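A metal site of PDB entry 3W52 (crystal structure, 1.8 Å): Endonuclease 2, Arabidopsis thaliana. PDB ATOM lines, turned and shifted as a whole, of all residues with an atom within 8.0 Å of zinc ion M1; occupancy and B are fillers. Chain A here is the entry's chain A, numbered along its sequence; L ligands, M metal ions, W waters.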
ATOM      1  N   TRP A   1     -13.792  23.795  -3.738  1.00  0.00           N
ATOM      2  CA  TRP A   1     -13.567  24.773  -4.843  1.00  0.00           C
ATOM      3  C   TRP A   1     -12.157  24.624  -5.383  1.00  0.00           C
ATOM      4  O   TRP A   1     -11.287  24.054  -4.722  1.00  0.00           O
ATOM      5  CB  TRP A   1     -13.642  26.237  -4.281  1.00  0.00           C
ATOM      6  CG  TRP A   1     -14.904  26.585  -3.504  1.00  0.00           C
ATOM      7  CD1 TRP A   1     -15.084  26.583  -2.129  1.00  0.00           C
ATOM      8  CD2 TRP A   1     -16.141  27.055  -4.082  1.00  0.00           C
ATOM      9  NE1 TRP A   1     -16.368  27.059  -1.826  1.00  0.00           N
ATOM     10  CE2 TRP A   1     -17.015  27.344  -2.986  1.00  0.00           C
ATOM     11  CE3 TRP A   1     -16.578  27.260  -5.374  1.00  0.00           C
ATOM     12  CZ2 TRP A   1     -18.323  27.820  -3.189  1.00  0.00           C
ATOM     13  CZ3 TRP A   1     -17.899  27.738  -5.592  1.00  0.00           C
ATOM     14  CH2 TRP A   1     -18.749  28.010  -4.493  1.00  0.00           C
ATOM     15  N   GLY A   2     -11.966  25.197  -6.560  1.00  0.00           N
ATOM     16  CA  GLY A   2     -10.623  25.292  -7.098  1.00  0.00           C
ATOM     17  C   GLY A   2      -9.886  26.478  -6.495  1.00  0.00           C
ATOM     18  O   GLY A   2     -10.306  27.126  -5.520  1.00  0.00           O
ATOM     19  N   HIS A   6     -11.146  29.346  -3.336  1.00  0.00           N
ATOM     20  CA  HIS A   6     -10.522  29.408  -2.007  1.00  0.00           C
ATOM     21  C   HIS A   6      -9.788  30.736  -1.812  1.00  0.00           C
ATOM     22  O   HIS A   6      -9.772  31.296  -0.715  1.00  0.00           O
ATOM     23  CB  HIS A   6      -9.506  28.252  -1.837  1.00  0.00           C
ATOM     24  CG  HIS A   6     -10.188  26.942  -1.617  1.00  0.00           C
ATOM     25  ND1 HIS A   6     -10.858  26.653  -0.442  1.00  0.00           N
ATOM     26  CD2 HIS A   6     -10.438  25.929  -2.467  1.00  0.00           C
ATOM     27  CE1 HIS A   6     -11.493  25.500  -0.577  1.00  0.00           C
ATOM     28  NE2 HIS A   6     -11.246  25.041  -1.800  1.00  0.00           N
ATOM     29  N   ASP A  45      -5.554  20.806  -0.463  1.00  0.00           N
ATOM     30  CA  ASP A  45      -5.717  19.947  -1.637  1.00  0.00           C
ATOM     31  C   ASP A  45      -4.374  19.275  -2.022  1.00  0.00           C
ATOM     32  O   ASP A  45      -4.379  18.194  -2.615  1.00  0.00           O
ATOM     33  CB  ASP A  45      -6.214  20.772  -2.821  1.00  0.00           C
ATOM     34  CG  ASP A  45      -7.724  20.906  -2.855  1.00  0.00           C
ATOM     35  OD1 ASP A  45      -8.460  20.283  -2.036  1.00  0.00           O
ATOM     36  OD2 ASP A  45      -8.199  21.639  -3.763  1.00  0.00           O
ATOM     37  N   LYS A  48      -3.724  15.668  -0.186  1.00  0.00           N
ATOM     38  CA  LYS A  48      -4.749  14.615  -0.295  1.00  0.00           C
ATOM     39  C   LYS A  48      -4.078  13.200  -0.437  1.00  0.00           C
ATOM     40  O   LYS A  48      -4.671  12.207  -0.046  1.00  0.00           O
ATOM     41  CB  LYS A  48      -5.584  14.844  -1.566  1.00  0.00           C
ATOM     42  CG  LYS A  48      -6.699  15.850  -1.373  1.00  0.00           C
ATOM     43  CD  LYS A  48      -7.518  16.046  -2.663  1.00  0.00           C
ATOM     44  CE  LYS A  48      -8.657  17.047  -2.315  1.00  0.00           C
ATOM     45  NZ  LYS A  48      -9.330  17.461  -3.580  1.00  0.00           N
ATOM     46  N   HIS A  58     -12.770  16.463   2.663  1.00  0.00           N
ATOM     47  CA  HIS A  58     -13.145  17.631   1.841  1.00  0.00           C
ATOM     48  C   HIS A  58     -14.600  17.698   1.477  1.00  0.00           C
ATOM     49  O   HIS A  58     -15.046  18.755   0.958  1.00  0.00           O
ATOM     50  CB  HIS A  58     -12.358  17.641   0.518  1.00  0.00           C
ATOM     51  CG  HIS A  58     -10.887  17.820   0.715  1.00  0.00           C
ATOM     52  ND1 HIS A  58     -10.219  18.949   0.264  1.00  0.00           N
ATOM     53  CD2 HIS A  58      -9.978  17.078   1.368  1.00  0.00           C
ATOM     54  CE1 HIS A  58      -8.954  18.881   0.634  1.00  0.00           C
ATOM     55  NE2 HIS A  58      -8.772  17.753   1.312  1.00  0.00           N
ATOM     56  N   TYR A  59     -15.374  16.635   1.737  1.00  0.00           N
ATOM     57  CA  TYR A  59     -16.768  16.704   1.279  1.00  0.00           C
ATOM     58  C   TYR A  59     -17.673  15.836   2.197  1.00  0.00           C
ATOM     59  O   TYR A  59     -17.190  15.321   3.199  1.00  0.00           O
ATOM     60  CB  TYR A  59     -16.885  16.180  -0.141  1.00  0.00           C
ATOM     61  CG  TYR A  59     -16.257  14.798  -0.280  1.00  0.00           C
ATOM     62  CD1 TYR A  59     -16.980  13.645   0.054  1.00  0.00           C
ATOM     63  CD2 TYR A  59     -14.926  14.657  -0.708  1.00  0.00           C
ATOM     64  CE1 TYR A  59     -16.414  12.369  -0.026  1.00  0.00           C
ATOM     65  CE2 TYR A  59     -14.351  13.372  -0.785  1.00  0.00           C
ATOM     66  CZ  TYR A  59     -15.112  12.259  -0.437  1.00  0.00           C
ATOM     67  OH  TYR A  59     -14.522  10.990  -0.552  1.00  0.00           O
ATOM     68  N   HIS A 120      -9.284  25.960   4.471  1.00  0.00           N
ATOM     69  CA  HIS A 120      -9.740  25.267   3.261  1.00  0.00           C
ATOM     70  C   HIS A 120     -11.139  24.579   3.447  1.00  0.00           C
ATOM     71  O   HIS A 120     -12.011  24.689   2.583  1.00  0.00           O
ATOM     72  CB  HIS A 120      -8.688  24.197   2.899  1.00  0.00           C
ATOM     73  CG  HIS A 120      -8.984  23.500   1.612  1.00  0.00           C
ATOM     74  ND1 HIS A 120      -8.502  23.966   0.402  1.00  0.00           N
ATOM     75  CD2 HIS A 120      -9.714  22.395   1.340  1.00  0.00           C
ATOM     76  CE1 HIS A 120      -8.937  23.172  -0.573  1.00  0.00           C
ATOM     77  NE2 HIS A 120      -9.675  22.214  -0.033  1.00  0.00           N
ATOM     78  N   ASP A 124     -14.631  24.593   1.455  1.00  0.00           N
ATOM     79  CA  ASP A 124     -15.247  23.460   0.778  1.00  0.00           C
ATOM     80  C   ASP A 124     -16.669  23.166   1.249  1.00  0.00           C
ATOM     81  O   ASP A 124     -17.497  22.753   0.454  1.00  0.00           O
ATOM     82  CB  ASP A 124     -14.354  22.222   0.951  1.00  0.00           C
ATOM     83  CG  ASP A 124     -13.283  22.108  -0.118  1.00  0.00           C
ATOM     84  OD1 ASP A 124     -13.234  22.991  -0.971  1.00  0.00           O
ATOM     85  OD2 ASP A 124     -12.533  21.121  -0.102  1.00  0.00           O
ATOM     86  N   GLN A 127     -19.213  24.848  -0.891  1.00  0.00           N
ATOM     87  CA  GLN A 127     -19.391  24.514  -2.336  1.00  0.00           C
ATOM     88  C   GLN A 127     -20.573  23.534  -2.320  1.00  0.00           C
ATOM     89  O   GLN A 127     -20.470  22.450  -1.728  1.00  0.00           O
ATOM     90  CB  GLN A 127     -18.061  23.843  -2.857  1.00  0.00           C
ATOM     91  CG  GLN A 127     -17.815  24.038  -4.370  1.00  0.00           C
ATOM     92  CD  GLN A 127     -18.683  23.155  -5.269  1.00  0.00           C
ATOM     93  OE1 GLN A 127     -19.872  23.222  -5.222  1.00  0.00           O
ATOM     94  NE2 GLN A 127     -18.051  22.333  -6.108  1.00  0.00           N
ATOM     95  N   LEU A 129     -21.781  21.322  -4.306  1.00  0.00           N
ATOM     96  CA  LEU A 129     -21.500  19.923  -4.677  1.00  0.00           C
ATOM     97  C   LEU A 129     -20.497  19.238  -3.789  1.00  0.00           C
ATOM     98  O   LEU A 129     -20.172  18.023  -4.009  1.00  0.00           O
ATOM     99  CB  LEU A 129     -21.135  19.812  -6.168  1.00  0.00           C
ATOM    100  CG  LEU A 129     -22.387  20.093  -7.017  1.00  0.00           C
ATOM    101  CD1 LEU A 129     -21.903  19.965  -8.509  1.00  0.00           C
ATOM    102  CD2 LEU A 129     -23.572  19.052  -6.738  1.00  0.00           C
ATOM    103  N   HIS A 130     -19.989  19.920  -2.761  1.00  0.00           N
ATOM    104  CA  HIS A 130     -19.212  19.183  -1.773  1.00  0.00           C
ATOM    105  C   HIS A 130     -20.126  18.614  -0.665  1.00  0.00           C
ATOM    106  O   HIS A 130     -19.628  18.003   0.281  1.00  0.00           O
ATOM    107  CB  HIS A 130     -18.130  20.038  -1.124  1.00  0.00           C
ATOM    108  CG  HIS A 130     -16.902  20.122  -1.979  1.00  0.00           C
ATOM    109  ND1 HIS A 130     -15.639  19.818  -1.521  1.00  0.00           N
ATOM    110  CD2 HIS A 130     -16.775  20.414  -3.290  1.00  0.00           C
ATOM    111  CE1 HIS A 130     -14.772  19.902  -2.513  1.00  0.00           C
ATOM    112  NE2 HIS A 130     -15.442  20.266  -3.601  1.00  0.00           N
ATOM    113  N   LYS A 137     -20.906  10.906  -7.049  1.00  0.00           N
ATOM    114  CA  LYS A 137     -19.640  11.399  -6.484  1.00  0.00           C
ATOM    115  C   LYS A 137     -19.636  12.904  -6.514  1.00  0.00           C
ATOM    116  O   LYS A 137     -18.690  13.524  -7.008  1.00  0.00           O
ATOM    117  CB  LYS A 137     -18.483  10.859  -7.305  1.00  0.00           C
ATOM    118  CG  LYS A 137     -18.374   9.296  -7.223  1.00  0.00           C
ATOM    119  CD  LYS A 137     -17.045   8.843  -7.779  1.00  0.00           C
ATOM    120  CE  LYS A 137     -17.056   7.348  -8.092  1.00  0.00           C
ATOM    121  NZ  LYS A 137     -17.870   7.003  -9.321  1.00  0.00           N
ATOM    122  N   GLY A 138     -20.721  13.468  -5.998  1.00  0.00           N
ATOM    123  CA  GLY A 138     -20.835  14.924  -5.930  1.00  0.00           C
ATOM    124  C   GLY A 138     -20.806  15.620  -7.280  1.00  0.00           C
ATOM    125  O   GLY A 138     -20.231  16.717  -7.423  1.00  0.00           O
ATOM    126  N   ASN A 140     -19.299  14.545  -9.872  1.00  0.00           N
ATOM    127  CA  ASN A 140     -18.092  14.259 -10.644  1.00  0.00           C
ATOM    128  C   ASN A 140     -18.331  13.312 -11.830  1.00  0.00           C
ATOM    129  O   ASN A 140     -17.589  13.369 -12.823  1.00  0.00           O
ATOM    130  CB  ASN A 140     -16.995  13.686  -9.741  1.00  0.00           C
ATOM    131  CG  ASN A 140     -16.177  14.777  -9.063  1.00  0.00           C
ATOM    132  OD1 ASN A 140     -15.343  15.445  -9.734  1.00  0.00           O
ATOM    133  ND2 ASN A 140     -16.402  14.982  -7.751  1.00  0.00           N
ATOM    134  N   ASN A 152     -17.125  18.090 -16.119  1.00  0.00           N
ATOM    135  CA  ASN A 152     -18.112  17.403 -15.274  1.00  0.00           C
ATOM    136  C   ASN A 152     -18.780  18.492 -14.415  1.00  0.00           C
ATOM    137  O   ASN A 152     -18.254  19.609 -14.215  1.00  0.00           O
ATOM    138  CB  ASN A 152     -17.516  16.248 -14.445  1.00  0.00           C
ATOM    139  CG  ASN A 152     -16.499  16.680 -13.492  1.00  0.00           C
ATOM    140  OD1 ASN A 152     -16.801  17.306 -12.505  1.00  0.00           O
ATOM    141  ND2 ASN A 152     -15.227  16.331 -13.765  1.00  0.00           N
ATOM    142  N   HIS A 154     -19.254  18.731 -11.228  1.00  0.00           N
ATOM    143  CA  HIS A 154     -18.521  19.097 -10.018  1.00  0.00           C
ATOM    144  C   HIS A 154     -17.475  20.177 -10.342  1.00  0.00           C
ATOM    145  O   HIS A 154     -17.381  21.184  -9.637  1.00  0.00           O
ATOM    146  CB  HIS A 154     -17.821  17.919  -9.366  1.00  0.00           C
ATOM    147  CG  HIS A 154     -17.227  18.250  -8.024  1.00  0.00           C
ATOM    148  ND1 HIS A 154     -17.885  18.041  -6.820  1.00  0.00           N
ATOM    149  CD2 HIS A 154     -16.066  18.873  -7.711  1.00  0.00           C
ATOM    150  CE1 HIS A 154     -17.139  18.510  -5.836  1.00  0.00           C
ATOM    151  NE2 HIS A 154     -16.035  19.031  -6.351  1.00  0.00           N
ATOM    152  N   HIS A 155     -16.734  19.965 -11.401  1.00  0.00           N
ATOM    153  CA  HIS A 155     -15.683  20.916 -11.817  1.00  0.00           C
ATOM    154  C   HIS A 155     -16.264  22.257 -12.240  1.00  0.00           C
ATOM    155  O   HIS A 155     -15.644  23.302 -12.054  1.00  0.00           O
ATOM    156  CB  HIS A 155     -14.877  20.267 -12.948  1.00  0.00           C
ATOM    157  CG  HIS A 155     -13.646  21.038 -13.323  1.00  0.00           C
ATOM    158  ND1 HIS A 155     -13.647  22.048 -14.260  1.00  0.00           N
ATOM    159  CD2 HIS A 155     -12.375  20.959 -12.851  1.00  0.00           C
ATOM    160  CE1 HIS A 155     -12.430  22.565 -14.351  1.00  0.00           C
ATOM    161  NE2 HIS A 155     -11.638  21.915 -13.512  1.00  0.00           N
ATOM    162  N   TRP A 157     -18.777  23.705 -10.852  1.00  0.00           N
ATOM    163  CA  TRP A 157     -18.958  24.461  -9.602  1.00  0.00           C
ATOM    164  C   TRP A 157     -17.657  24.772  -8.868  1.00  0.00           C
ATOM    165  O   TRP A 157     -17.517  25.826  -8.264  1.00  0.00           O
ATOM    166  CB  TRP A 157     -19.928  23.697  -8.649  1.00  0.00           C
ATOM    167  CG  TRP A 157     -21.343  23.928  -9.118  1.00  0.00           C
ATOM    168  CD1 TRP A 157     -21.950  23.351 -10.202  1.00  0.00           C
ATOM    169  CD2 TRP A 157     -22.263  24.893  -8.592  1.00  0.00           C
ATOM    170  NE1 TRP A 157     -23.228  23.940 -10.401  1.00  0.00           N
ATOM    171  CE2 TRP A 157     -23.420  24.871  -9.412  1.00  0.00           C
ATOM    172  CE3 TRP A 157     -22.209  25.801  -7.503  1.00  0.00           C
ATOM    173  CZ2 TRP A 157     -24.510  25.720  -9.184  1.00  0.00           C
ATOM    174  CZ3 TRP A 157     -23.253  26.639  -7.278  1.00  0.00           C
ATOM    175  CH2 TRP A 157     -24.405  26.603  -8.117  1.00  0.00           C
ATOM    176  N   ASP A 158     -16.668  23.888  -8.902  1.00  0.00           N
ATOM    177  CA  ASP A 158     -15.413  24.229  -8.190  1.00  0.00           C
ATOM    178  C   ASP A 158     -14.683  25.356  -8.940  1.00  0.00           C
ATOM    179  O   ASP A 158     -14.067  26.206  -8.320  1.00  0.00           O
ATOM    180  CB  ASP A 158     -14.403  23.062  -8.272  1.00  0.00           C
ATOM    181  CG  ASP A 158     -14.533  22.047  -7.124  1.00  0.00           C
ATOM    182  OD1 ASP A 158     -15.224  22.304  -6.129  1.00  0.00           O
ATOM    183  OD2 ASP A 158     -13.886  20.965  -7.274  1.00  0.00           O
ATOM    184  N   SER A 159     -14.738  25.268 -10.268  1.00  0.00           N
ATOM    185  CA  SER A 159     -13.925  26.170 -11.125  1.00  0.00           C
ATOM    186  C   SER A 159     -14.499  26.907 -12.322  1.00  0.00           C
ATOM    187  O   SER A 159     -14.269  28.133 -12.434  1.00  0.00           O
ATOM    188  CB  SER A 159     -12.727  25.382 -11.642  1.00  0.00           C
ATOM    189  OG  SER A 159     -11.873  24.898 -10.590  1.00  0.00           O
HETATM  190  S1  LIG L   1     -11.432  20.557  -3.792  1.00  0.00           S
HETATM  191  O1  LIG L   1     -11.172  21.664  -2.802  1.00  0.00           O
HETATM  192  O2  LIG L   1     -11.471  19.265  -2.942  1.00  0.00           O
HETATM  193  O3  LIG L   1     -12.630  20.815  -4.572  1.00  0.00           O
HETATM  194  O4  LIG L   1     -10.203  20.556  -4.715  1.00  0.00           O
HETATM  195  N1  LG2 L   2     -14.794  15.910  -4.509  1.00  0.00           N
HETATM  196  C1  LG2 L   2     -13.925  14.854  -4.746  1.00  0.00           C
HETATM  197  N2  LG2 L   2     -14.482  13.671  -4.564  1.00  0.00           N
HETATM  198  C2  LG2 L   2     -15.785  13.963  -4.179  1.00  0.00           C
HETATM  199  C3  LG2 L   2     -16.858  13.144  -3.844  1.00  0.00           C
HETATM  200  N3  LG2 L   2     -16.780  11.814  -3.861  1.00  0.00           N
HETATM  201  N4  LG2 L   2     -18.022  13.729  -3.497  1.00  0.00           N
HETATM  202  C4  LG2 L   2     -18.084  15.097  -3.488  1.00  0.00           C
HETATM  203  N5  LG2 L   2     -17.134  15.974  -3.785  1.00  0.00           N
HETATM  204  C5  LG2 L   2     -15.991  15.337  -4.122  1.00  0.00           C
HETATM  205 ZN    ZN M   1     -14.371  20.018  -5.433  1.00  0.00          ZN
HETATM  206 ZN    ZN M   2     -12.094  23.440  -2.677  1.00  0.00          ZN
HETATM  207 ZN    ZN M   3     -10.717  20.630  -1.018  1.00  0.00          ZN
HETATM  208  O   HOH W   1     -13.215  18.178  -5.600  1.00  0.00           O
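O of His 58 lies within hydrogen-bond range of ND1 of His 130 (2.8 Å).
O of Asp 158 sits at hydrogen-bond distance from N of Gly 2, 2.9 Å away.
The backbone NH (N) of His 154 sits at hydrogen-bond distance from the side-chain amide oxygen (OD1) of Asn 152 (3.1 Å).
O of Gly 138 lies within hydrogen-bond range of ND1 of His 154.
The side-chain amide nitrogen (NE2) of Gln 127 lies close to the backbone NH (N) of Asp 158.
Within 4 Å of zinc ion M1: His 130, His 154 and Asp 158.
Along chain A the residues within 4 Å of zinc ion M1 span positions 130 to 158.
Zinc ion M1 is bound by an oxygen (O3) of LIG L1 (2.1 Å), the side-chain carboxylate (OD2) of Asp 158 (2.1 Å), a ring nitrogen (NE2) of His 130 (2.1 Å), a ring nitrogen (NE2) of His 154 (2.1 Å), water W1 (2.2 Å) and the side-chain carboxylate (OD1) of Asp 158 (2.5 Å).
Zinc ion M1 has six donor atoms within binding distance.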
